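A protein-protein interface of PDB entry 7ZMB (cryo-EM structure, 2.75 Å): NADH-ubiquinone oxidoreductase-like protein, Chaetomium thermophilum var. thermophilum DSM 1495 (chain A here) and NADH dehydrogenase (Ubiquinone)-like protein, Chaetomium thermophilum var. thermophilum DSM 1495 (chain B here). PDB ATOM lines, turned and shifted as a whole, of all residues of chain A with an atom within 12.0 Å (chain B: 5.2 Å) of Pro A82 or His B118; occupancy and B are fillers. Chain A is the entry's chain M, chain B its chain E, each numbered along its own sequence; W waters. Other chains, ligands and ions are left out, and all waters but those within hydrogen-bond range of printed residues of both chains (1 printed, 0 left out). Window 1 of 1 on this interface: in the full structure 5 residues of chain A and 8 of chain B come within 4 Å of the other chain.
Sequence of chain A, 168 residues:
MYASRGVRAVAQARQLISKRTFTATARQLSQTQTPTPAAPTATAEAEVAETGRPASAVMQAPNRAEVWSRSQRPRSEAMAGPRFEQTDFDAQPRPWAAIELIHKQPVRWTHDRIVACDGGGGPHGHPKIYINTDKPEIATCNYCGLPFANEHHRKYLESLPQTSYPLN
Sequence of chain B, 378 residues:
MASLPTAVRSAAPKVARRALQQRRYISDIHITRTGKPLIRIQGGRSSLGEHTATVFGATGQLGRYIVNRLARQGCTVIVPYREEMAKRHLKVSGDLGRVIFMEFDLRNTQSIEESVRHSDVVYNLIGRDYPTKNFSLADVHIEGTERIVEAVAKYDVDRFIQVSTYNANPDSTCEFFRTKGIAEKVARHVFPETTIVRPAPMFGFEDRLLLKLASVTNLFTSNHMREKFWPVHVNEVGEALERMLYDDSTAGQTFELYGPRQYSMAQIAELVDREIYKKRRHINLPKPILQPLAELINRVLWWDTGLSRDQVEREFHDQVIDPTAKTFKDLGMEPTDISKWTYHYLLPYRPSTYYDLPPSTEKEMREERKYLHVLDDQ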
ATOM      1  N   GLY A  52      -7.511  29.869 -13.386  1.00  0.00           N
ATOM      2  CA  GLY A  52      -8.446  30.707 -14.113  1.00  0.00           C
ATOM      3  C   GLY A  52      -7.773  31.703 -15.037  1.00  0.00           C
ATOM      4  O   GLY A  52      -8.156  32.872 -15.090  1.00  0.00           O
ATOM      5  N   ARG A  53      -6.762  31.240 -15.768  1.00  0.00           N
ATOM      6  CA  ARG A  53      -6.017  32.101 -16.677  1.00  0.00           C
ATOM      7  C   ARG A  53      -6.771  32.362 -17.983  1.00  0.00           C
ATOM      8  O   ARG A  53      -6.978  33.528 -18.335  1.00  0.00           O
ATOM      9  CB  ARG A  53      -4.636  31.503 -16.964  1.00  0.00           C
ATOM     10  CG  ARG A  53      -3.660  32.482 -17.590  1.00  0.00           C
ATOM     11  CD  ARG A  53      -3.537  33.742 -16.752  1.00  0.00           C
ATOM     12  NE  ARG A  53      -2.617  34.706 -17.348  1.00  0.00           N
ATOM     13  CZ  ARG A  53      -2.420  35.935 -16.884  1.00  0.00           C
ATOM     14  NH1 ARG A  53      -3.081  36.355 -15.814  1.00  0.00           N
ATOM     15  NH2 ARG A  53      -1.563  36.746 -17.489  1.00  0.00           N
ATOM     16  N   PRO A  54      -7.197  31.342 -18.731  1.00  0.00           N
ATOM     17  CA  PRO A  54      -7.823  31.605 -20.029  1.00  0.00           C
ATOM     18  C   PRO A  54      -9.254  32.097 -19.880  1.00  0.00           C
ATOM     19  O   PRO A  54      -9.889  31.965 -18.833  1.00  0.00           O
ATOM     20  CB  PRO A  54      -7.794  30.240 -20.731  1.00  0.00           C
ATOM     21  CG  PRO A  54      -7.079  29.310 -19.804  1.00  0.00           C
ATOM     22  CD  PRO A  54      -7.206  29.899 -18.446  1.00  0.00           C
ATOM     23  N   ALA A  57     -11.953  29.333 -19.137  1.00  0.00           N
ATOM     24  CA  ALA A  57     -11.987  28.814 -17.764  1.00  0.00           C
ATOM     25  C   ALA A  57     -12.686  29.856 -16.901  1.00  0.00           C
ATOM     26  O   ALA A  57     -12.896  29.594 -15.710  1.00  0.00           O
ATOM     27  CB  ALA A  57     -10.579  28.606 -17.315  1.00  0.00           C
ATOM     28  N   ARG A  73     -22.913  27.689 -10.029  1.00  0.00           N
ATOM     29  CA  ARG A  73     -21.564  28.000  -9.615  1.00  0.00           C
ATOM     30  C   ARG A  73     -20.817  28.603 -10.797  1.00  0.00           C
ATOM     31  O   ARG A  73     -20.810  28.013 -11.881  1.00  0.00           O
ATOM     32  CB  ARG A  73     -20.867  26.749  -9.108  1.00  0.00           C
ATOM     33  CG  ARG A  73     -19.482  26.968  -8.537  1.00  0.00           C
ATOM     34  CD  ARG A  73     -18.849  25.635  -8.206  1.00  0.00           C
ATOM     35  NE  ARG A  73     -17.516  25.758  -7.631  1.00  0.00           N
ATOM     36  CZ  ARG A  73     -16.762  24.721  -7.283  1.00  0.00           C
ATOM     37  NH1 ARG A  73     -15.559  24.918  -6.766  1.00  0.00           N
ATOM     38  NH2 ARG A  73     -17.201  23.484  -7.476  1.00  0.00           N
ATOM     39  N   ARG A  75     -17.966  29.559 -13.507  1.00  0.00           N
ATOM     40  CA  ARG A  75     -16.925  28.652 -14.057  1.00  0.00           C
ATOM     41  C   ARG A  75     -15.583  28.945 -13.379  1.00  0.00           C
ATOM     42  O   ARG A  75     -14.880  27.983 -13.066  1.00  0.00           O
ATOM     43  CB  ARG A  75     -16.881  28.708 -15.590  1.00  0.00           C
ATOM     44  CG  ARG A  75     -15.970  27.661 -16.208  1.00  0.00           C
ATOM     45  CD  ARG A  75     -16.012  27.612 -17.719  1.00  0.00           C
ATOM     46  NE  ARG A  75     -17.230  27.000 -18.227  1.00  0.00           N
ATOM     47  CZ  ARG A  75     -17.358  25.713 -18.526  1.00  0.00           C
ATOM     48  NH1 ARG A  75     -18.506  25.254 -18.989  1.00  0.00           N
ATOM     49  NH2 ARG A  75     -16.338  24.890 -18.362  1.00  0.00           N
ATOM     50  N   SER A  76     -15.267  30.216 -13.145  1.00  0.00           N
ATOM     51  CA  SER A  76     -14.003  30.627 -12.484  1.00  0.00           C
ATOM     52  C   SER A  76     -13.931  30.056 -11.066  1.00  0.00           C
ATOM     53  O   SER A  76     -12.813  29.844 -10.572  1.00  0.00           O
ATOM     54  CB  SER A  76     -13.903  32.113 -12.456  1.00  0.00           C
ATOM     55  OG  SER A  76     -15.014  32.674 -11.774  1.00  0.00           O
ATOM     56  N   GLU A  77     -15.084  29.813 -10.437  1.00  0.00           N
ATOM     57  CA  GLU A  77     -15.095  29.245  -9.099  1.00  0.00           C
ATOM     58  C   GLU A  77     -15.099  27.724  -9.103  1.00  0.00           C
ATOM     59  O   GLU A  77     -15.007  27.117  -8.035  1.00  0.00           O
ATOM     60  CB  GLU A  77     -16.304  29.755  -8.321  1.00  0.00           C
ATOM     61  CG  GLU A  77     -16.318  31.247  -8.116  1.00  0.00           C
ATOM     62  CD  GLU A  77     -17.488  31.701  -7.267  1.00  0.00           C
ATOM     63  OE1 GLU A  77     -18.094  30.850  -6.578  1.00  0.00           O
ATOM     64  OE2 GLU A  77     -17.809  32.907  -7.293  1.00  0.00           O
ATOM     65  N   ALA A  78     -15.198  27.093 -10.268  1.00  0.00           N
ATOM     66  CA  ALA A  78     -15.197  25.643 -10.353  1.00  0.00           C
ATOM     67  C   ALA A  78     -14.045  25.075 -11.165  1.00  0.00           C
ATOM     68  O   ALA A  78     -13.771  23.879 -11.048  1.00  0.00           O
ATOM     69  CB  ALA A  78     -16.524  25.143 -10.940  1.00  0.00           C
ATOM     70  N   MET A  79     -13.367  25.889 -11.976  1.00  0.00           N
ATOM     71  CA  MET A  79     -12.118  25.518 -12.630  1.00  0.00           C
ATOM     72  C   MET A  79     -10.903  25.774 -11.755  1.00  0.00           C
ATOM     73  O   MET A  79      -9.777  25.661 -12.240  1.00  0.00           O
ATOM     74  CB  MET A  79     -11.922  26.295 -13.939  1.00  0.00           C
ATOM     75  CG  MET A  79     -13.015  26.209 -14.979  1.00  0.00           C
ATOM     76  SD  MET A  79     -13.129  24.645 -15.845  1.00  0.00           S
ATOM     77  CE  MET A  79     -14.512  23.958 -14.980  1.00  0.00           C
ATOM     78  N   ALA A  80     -11.088  26.163 -10.505  1.00  0.00           N
ATOM     79  CA  ALA A  80      -9.957  26.402  -9.625  1.00  0.00           C
ATOM     80  C   ALA A  80      -9.721  25.190  -8.734  1.00  0.00           C
ATOM     81  O   ALA A  80     -10.598  24.349  -8.542  1.00  0.00           O
ATOM     82  CB  ALA A  80     -10.184  27.650  -8.775  1.00  0.00           C
ATOM     83  N   GLY A  81      -8.513  25.100  -8.199  1.00  0.00           N
ATOM     84  CA  GLY A  81      -8.174  24.018  -7.312  1.00  0.00           C
ATOM     85  C   GLY A  81      -7.103  23.108  -7.867  1.00  0.00           C
ATOM     86  O   GLY A  81      -6.688  23.229  -9.022  1.00  0.00           O
ATOM     87  N   PRO A  82      -6.620  22.184  -7.034  1.00  0.00           N
ATOM     88  CA  PRO A  82      -5.547  21.284  -7.482  1.00  0.00           C
ATOM     89  C   PRO A  82      -5.944  20.419  -8.658  1.00  0.00           C
ATOM     90  O   PRO A  82      -5.090  20.066  -9.477  1.00  0.00           O
ATOM     91  CB  PRO A  82      -5.250  20.437  -6.235  1.00  0.00           C
ATOM     92  CG  PRO A  82      -5.975  21.076  -5.114  1.00  0.00           C
ATOM     93  CD  PRO A  82      -7.086  21.874  -5.675  1.00  0.00           C
ATOM     94  N   ARG A  83      -7.228  20.116  -8.789  1.00  0.00           N
ATOM     95  CA  ARG A  83      -7.681  19.211  -9.870  1.00  0.00           C
ATOM     96  C   ARG A  83      -7.577  19.914 -11.225  1.00  0.00           C
ATOM     97  O   ARG A  83      -7.818  19.260 -12.242  1.00  0.00           O
ATOM     98  CB  ARG A  83      -9.113  18.782  -9.560  1.00  0.00           C
ATOM     99  CG  ARG A  83      -9.231  17.857  -8.358  1.00  0.00           C
ATOM    100  CD  ARG A  83     -10.561  17.136  -8.317  1.00  0.00           C
ATOM    101  NE  ARG A  83     -11.676  18.065  -8.435  1.00  0.00           N
ATOM    102  CZ  ARG A  83     -12.491  18.152  -9.480  1.00  0.00           C
ATOM    103  NH1 ARG A  83     -13.469  19.040  -9.473  1.00  0.00           N
ATOM    104  NH2 ARG A  83     -12.340  17.347 -10.515  1.00  0.00           N
ATOM    105  N   PHE A  84      -7.223  21.198 -11.233  1.00  0.00           N
ATOM    106  CA  PHE A  84      -7.169  21.986 -12.489  1.00  0.00           C
ATOM    107  C   PHE A  84      -5.766  22.558 -12.715  1.00  0.00           C
ATOM    108  O   PHE A  84      -5.684  23.643 -13.310  1.00  0.00           O
ATOM    109  CB  PHE A  84      -8.295  23.018 -12.414  1.00  0.00           C
ATOM    110  CG  PHE A  84      -9.679  22.426 -12.478  1.00  0.00           C
ATOM    111  CD1 PHE A  84     -10.289  22.184 -13.698  1.00  0.00           C
ATOM    112  CD2 PHE A  84     -10.368  22.098 -11.321  1.00  0.00           C
ATOM    113  CE1 PHE A  84     -11.557  21.632 -13.760  1.00  0.00           C
ATOM    114  CE2 PHE A  84     -11.634  21.539 -11.385  1.00  0.00           C
ATOM    115  CZ  PHE A  84     -12.228  21.311 -12.604  1.00  0.00           C
ATOM    116  N   GLU A  85      -4.696  21.859 -12.326  1.00  0.00           N
ATOM    117  CA  GLU A  85      -3.363  22.438 -12.374  1.00  0.00           C
ATOM    118  C   GLU A  85      -2.520  21.988 -13.555  1.00  0.00           C
ATOM    119  O   GLU A  85      -1.504  22.634 -13.844  1.00  0.00           O
ATOM    120  CB  GLU A  85      -2.608  22.139 -11.081  1.00  0.00           C
ATOM    121  CG  GLU A  85      -2.946  23.112  -9.992  1.00  0.00           C
ATOM    122  CD  GLU A  85      -2.615  24.526 -10.384  1.00  0.00           C
ATOM    123  OE1 GLU A  85      -1.508  24.745 -10.901  1.00  0.00           O
ATOM    124  OE2 GLU A  85      -3.461  25.417 -10.189  1.00  0.00           O
ATOM    125  N   GLN A  86      -2.895  20.914 -14.242  1.00  0.00           N
ATOM    126  CA  GLN A  86      -2.217  20.505 -15.466  1.00  0.00           C
ATOM    127  C   GLN A  86      -3.286  20.140 -16.495  1.00  0.00           C
ATOM    128  O   GLN A  86      -3.338  19.040 -17.030  1.00  0.00           O
ATOM    129  CB  GLN A  86      -1.235  19.366 -15.197  1.00  0.00           C
ATOM    130  CG  GLN A  86       0.074  19.843 -14.575  1.00  0.00           C
ATOM    131  CD  GLN A  86       0.906  18.714 -14.022  1.00  0.00           C
ATOM    132  OE1 GLN A  86       0.461  17.574 -13.969  1.00  0.00           O
ATOM    133  NE2 GLN A  86       2.120  19.024 -13.600  1.00  0.00           N
ATOM    134  N   THR A  87      -4.205  21.072 -16.727  1.00  0.00           N
ATOM    135  CA  THR A  87      -5.419  20.817 -17.483  1.00  0.00           C
ATOM    136  C   THR A  87      -5.511  21.748 -18.684  1.00  0.00           C
ATOM    137  O   THR A  87      -5.212  22.940 -18.583  1.00  0.00           O
ATOM    138  CB  THR A  87      -6.650  20.985 -16.580  1.00  0.00           C
ATOM    139  OG1 THR A  87      -6.512  20.138 -15.434  1.00  0.00           O
ATOM    140  CG2 THR A  87      -7.921  20.620 -17.315  1.00  0.00           C
ATOM    141  N   ASP A  88      -5.987  21.225 -19.825  1.00  0.00           N
ATOM    142  CA  ASP A  88      -6.259  22.077 -21.010  1.00  0.00           C
ATOM    143  C   ASP A  88      -7.691  22.608 -20.885  1.00  0.00           C
ATOM    144  O   ASP A  88      -8.618  21.804 -21.008  1.00  0.00           O
ATOM    145  CB  ASP A  88      -6.130  21.262 -22.284  1.00  0.00           C
ATOM    146  CG  ASP A  88      -6.093  22.114 -23.538  1.00  0.00           C
ATOM    147  OD1 ASP A  88      -5.734  23.303 -23.425  1.00  0.00           O
ATOM    148  OD2 ASP A  88      -6.424  21.586 -24.618  1.00  0.00           O
ATOM    149  N   PHE A  89      -7.847  23.923 -20.687  1.00  0.00           N
ATOM    150  CA  PHE A  89      -9.174  24.529 -20.415  1.00  0.00           C
ATOM    151  C   PHE A  89     -10.113  24.483 -21.613  1.00  0.00           C
ATOM    152  O   PHE A  89     -11.319  24.371 -21.408  1.00  0.00           O
ATOM    153  CB  PHE A  89      -9.019  25.878 -19.718  1.00  0.00           C
ATOM    154  CG  PHE A  89      -8.658  25.761 -18.259  1.00  0.00           C
ATOM    155  CD1 PHE A  89      -9.549  25.209 -17.353  1.00  0.00           C
ATOM    156  CD2 PHE A  89      -7.429  26.191 -17.792  1.00  0.00           C
ATOM    157  CE1 PHE A  89      -9.220  25.096 -16.012  1.00  0.00           C
ATOM    158  CE2 PHE A  89      -7.100  26.074 -16.452  1.00  0.00           C
ATOM    159  CZ  PHE A  89      -7.997  25.528 -15.565  1.00  0.00           C
ATOM    160  N   GLN A  92     -12.036  21.286 -22.230  1.00  0.00           N
ATOM    161  CA  GLN A  92     -13.057  20.943 -21.218  1.00  0.00           C
ATOM    162  C   GLN A  92     -14.420  21.094 -21.868  1.00  0.00           C
ATOM    163  O   GLN A  92     -14.522  21.863 -22.828  1.00  0.00           O
ATOM    164  CB  GLN A  92     -12.824  21.770 -19.954  1.00  0.00           C
ATOM    165  CG  GLN A  92     -11.544  21.394 -19.224  1.00  0.00           C
ATOM    166  CD  GLN A  92     -11.480  19.914 -18.936  1.00  0.00           C
ATOM    167  OE1 GLN A  92     -12.347  19.353 -18.272  1.00  0.00           O
ATOM    168  NE2 GLN A  92     -10.442  19.269 -19.438  1.00  0.00           N
ATOM    169  N   THR B  52      -5.428  20.645   2.383  1.00  0.00           N
ATOM    170  CA  THR B  52      -4.825  20.357   1.089  1.00  0.00           C
ATOM    171  C   THR B  52      -3.318  20.287   1.288  1.00  0.00           C
ATOM    172  O   THR B  52      -2.662  21.314   1.491  1.00  0.00           O
ATOM    173  CB  THR B  52      -5.199  21.400   0.037  1.00  0.00           C
ATOM    174  OG1 THR B  52      -6.616  21.407  -0.156  1.00  0.00           O
ATOM    175  CG2 THR B  52      -4.545  21.070  -1.277  1.00  0.00           C
ATOM    176  N   THR B  76      -7.245  16.363   0.648  1.00  0.00           N
ATOM    177  CA  THR B  76      -6.702  16.402  -0.700  1.00  0.00           C
ATOM    178  C   THR B  76      -5.181  16.385  -0.648  1.00  0.00           C
ATOM    179  O   THR B  76      -4.563  17.207   0.030  1.00  0.00           O
ATOM    180  CB  THR B  76      -7.208  17.640  -1.436  1.00  0.00           C
ATOM    181  OG1 THR B  76      -8.602  17.488  -1.718  1.00  0.00           O
ATOM    182  CG2 THR B  76      -6.458  17.857  -2.711  1.00  0.00           C
ATOM    183  N   ILE B  78      -1.764  16.309  -3.030  1.00  0.00           N
ATOM    184  CA  ILE B  78      -1.033  16.398  -4.291  1.00  0.00           C
ATOM    185  C   ILE B  78       0.228  15.553  -4.190  1.00  0.00           C
ATOM    186  O   ILE B  78       1.011  15.694  -3.245  1.00  0.00           O
ATOM    187  CB  ILE B  78      -0.700  17.857  -4.657  1.00  0.00           C
ATOM    188  CG1 ILE B  78      -1.963  18.678  -4.938  1.00  0.00           C
ATOM    189  CG2 ILE B  78       0.232  17.913  -5.851  1.00  0.00           C
ATOM    190  CD1 ILE B  78      -2.560  19.359  -3.777  1.00  0.00           C
ATOM    191  N   ILE B 100      -4.346  13.675  -5.998  1.00  0.00           N
ATOM    192  CA  ILE B 100      -4.102  14.304  -7.289  1.00  0.00           C
ATOM    193  C   ILE B 100      -2.637  14.119  -7.631  1.00  0.00           C
ATOM    194  O   ILE B 100      -1.757  14.514  -6.862  1.00  0.00           O
ATOM    195  CB  ILE B 100      -4.477  15.796  -7.283  1.00  0.00           C
ATOM    196  CG1 ILE B 100      -5.976  15.976  -7.097  1.00  0.00           C
ATOM    197  CG2 ILE B 100      -4.059  16.450  -8.566  1.00  0.00           C
ATOM    198  CD1 ILE B 100      -6.401  16.084  -5.673  1.00  0.00           C
ATOM    199  N   MET B 102       0.586  14.967  -9.910  1.00  0.00           N
ATOM    200  CA  MET B 102       1.177  15.987 -10.758  1.00  0.00           C
ATOM    201  C   MET B 102       2.530  15.465 -11.197  1.00  0.00           C
ATOM    202  O   MET B 102       3.260  14.885 -10.395  1.00  0.00           O
ATOM    203  CB  MET B 102       1.327  17.323 -10.028  1.00  0.00           C
ATOM    204  CG  MET B 102       0.013  18.026  -9.781  1.00  0.00           C
ATOM    205  SD  MET B 102      -0.338  19.345 -10.937  1.00  0.00           S
ATOM    206  CE  MET B 102       0.916  20.501 -10.452  1.00  0.00           C
ATOM    207  N   GLU B 114       3.380  24.785  -9.392  1.00  0.00           N
ATOM    208  CA  GLU B 114       2.020  24.355  -9.665  1.00  0.00           C
ATOM    209  C   GLU B 114       1.518  23.368  -8.628  1.00  0.00           C
ATOM    210  O   GLU B 114       0.305  23.179  -8.508  1.00  0.00           O
ATOM    211  CB  GLU B 114       1.933  23.719 -11.049  1.00  0.00           C
ATOM    212  CG  GLU B 114       2.137  24.660 -12.205  1.00  0.00           C
ATOM    213  CD  GLU B 114       2.435  23.920 -13.492  1.00  0.00           C
ATOM    214  OE1 GLU B 114       2.789  22.729 -13.419  1.00  0.00           O
ATOM    215  OE2 GLU B 114       2.303  24.525 -14.578  1.00  0.00           O
ATOM    216  N   VAL B 116       2.352  23.230  -5.132  1.00  0.00           N
ATOM    217  CA  VAL B 116       2.272  23.665  -3.744  1.00  0.00           C
ATOM    218  C   VAL B 116       1.376  24.872  -3.551  1.00  0.00           C
ATOM    219  O   VAL B 116       1.228  25.339  -2.415  1.00  0.00           O
ATOM    220  CB  VAL B 116       3.671  23.959  -3.169  1.00  0.00           C
ATOM    221  CG1 VAL B 116       4.521  22.719  -3.194  1.00  0.00           C
ATOM    222  CG2 VAL B 116       4.335  25.063  -3.963  1.00  0.00           C
ATOM    223  N   ARG B 117       0.780  25.403  -4.610  1.00  0.00           N
ATOM    224  CA  ARG B 117       0.141  26.706  -4.508  1.00  0.00           C
ATOM    225  C   ARG B 117      -1.315  26.643  -4.070  1.00  0.00           C
ATOM    226  O   ARG B 117      -1.905  27.691  -3.795  1.00  0.00           O
ATOM    227  CB  ARG B 117       0.262  27.449  -5.838  1.00  0.00           C
ATOM    228  CG  ARG B 117      -0.571  26.908  -6.951  1.00  0.00           C
ATOM    229  CD  ARG B 117      -0.395  27.789  -8.153  1.00  0.00           C
ATOM    230  NE  ARG B 117      -0.648  27.098  -9.408  1.00  0.00           N
ATOM    231  CZ  ARG B 117       0.083  27.261 -10.501  1.00  0.00           C
ATOM    232  NH1 ARG B 117       1.115  28.088 -10.491  1.00  0.00           N
ATOM    233  NH2 ARG B 117      -0.225  26.602 -11.606  1.00  0.00           N
ATOM    234  N   HIS B 118      -1.903  25.458  -3.990  1.00  0.00           N
ATOM    235  CA  HIS B 118      -3.246  25.297  -3.457  1.00  0.00           C
ATOM    236  C   HIS B 118      -3.232  24.744  -2.044  1.00  0.00           C
ATOM    237  O   HIS B 118      -4.281  24.359  -1.526  1.00  0.00           O
ATOM    238  CB  HIS B 118      -4.066  24.391  -4.372  1.00  0.00           C
ATOM    239  CG  HIS B 118      -4.398  25.013  -5.685  1.00  0.00           C
ATOM    240  ND1 HIS B 118      -5.011  26.240  -5.791  1.00  0.00           N
ATOM    241  CD2 HIS B 118      -4.170  24.595  -6.951  1.00  0.00           C
ATOM    242  CE1 HIS B 118      -5.162  26.545  -7.065  1.00  0.00           C
ATOM    243  NE2 HIS B 118      -4.657  25.566  -7.790  1.00  0.00           N
ATOM    244  N   SER B 119      -2.068  24.722  -1.406  1.00  0.00           N
ATOM    245  CA  SER B 119      -1.801  23.864  -0.266  1.00  0.00           C
ATOM    246  C   SER B 119      -1.690  24.663   1.020  1.00  0.00           C
ATOM    247  O   SER B 119      -1.320  25.837   1.018  1.00  0.00           O
ATOM    248  CB  SER B 119      -0.516  23.071  -0.490  1.00  0.00           C
ATOM    249  OG  SER B 119      -0.756  21.956  -1.318  1.00  0.00           O
ATOM    250  N   ASP B 120      -2.035  24.006   2.122  1.00  0.00           N
ATOM    251  CA  ASP B 120      -1.809  24.528   3.455  1.00  0.00           C
ATOM    252  C   ASP B 120      -0.713  23.782   4.202  1.00  0.00           C
ATOM    253  O   ASP B 120      -0.404  24.140   5.343  1.00  0.00           O
ATOM    254  CB  ASP B 120      -3.120  24.505   4.254  1.00  0.00           C
ATOM    255  CG  ASP B 120      -3.753  23.120   4.347  1.00  0.00           C
ATOM    256  OD1 ASP B 120      -3.060  22.102   4.183  1.00  0.00           O
ATOM    257  OD2 ASP B 120      -4.980  23.054   4.553  1.00  0.00           O
HETATM  258  O   HOH W   1      -2.640  20.046  -8.489  1.00  0.00           O
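Ala A57 touches none of the printed residues of chain B. Printed residues of chain B within 4 Å of Gly A81: His B118. Pro A82 touches three residues of chain B. Of the printed residues of chain B, Gln A86 touches Met B102 (3.4 Å) and Glu B114 (3.8 Å). No residue of chain A comes within 4 Å of Thr B76. Of the printed residues of chain A, Ile B78 touches Pro A82. Of the printed residues of chain A, Glu B114 touches Glu A85 and Gln A86. No residue of chain A comes within 4 Å of Val B116. Of chain A, only Glu A85 (2.4 Å) comes within 4 Å of Arg B117. Of chain A, only Gly A81 (3.3 Å), Pro A82 (3.4 Å) and Glu A85 (2.7 Å) come within 4 Å of His B118. No residue of chain A comes within 4 Å of Asp B120. The nearest residue of chain A that does not touch His B118 is Ala A80 (5.0 Å). The nearest printed residue of chain B that does not touch Arg A83 is His B118 (5.7 Å).
The side-chain amide oxygen of Gln A86 sits close to the side-chain sulfur of Met B102 (3.6 Å). OE1 of Glu A85 is in salt-bridge range of NE of Arg B117. NE2 of His B118 lies within hydrogen-bond range of O of Gly A81. The side-chain carboxylate (OE2) of Glu A85 sits at hydrogen-bond distance from a ring nitrogen (NE2) of His B118 (2.7 Å). The side-chain carboxylate of Glu A85 sits close to the backbone carbonyl oxygen of Glu B114 (3.4 Å).
Water W1 lies within hydrogen-bond range of the backbone carbonyl oxygen (O) of Pro A82 and the side-chain sulfur (SD) of Met B102.
Hydrophobic or aromatic side chains of chain A that line the printed part of chain B: Pro A82. Of the 11 printed residues of chain B, 6 touch a printed residue of chain A. Printed residues of chain B that touch a printed residue of chain A: Ile B78, Ile B100, Met B102, Glu B114, Arg B117 and His B118. Hydrophobic or aromatic side chains of chain B that line the printed part of chain A: Ile B78, Ile B100, Met B102 and His B118. Among the printed residues, 11 pairs touch across the chains.
CD1 of Ile B78 touches CB of Pro A82, 3.8 Å away. Ile B100 touches Pro A82. His B118 touches Pro A82. CG1 of Ile B100 touches CG of Arg A83, at 3.97 Å. Glu A85 touches Met B102. Glu B114 touches Gln A86.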
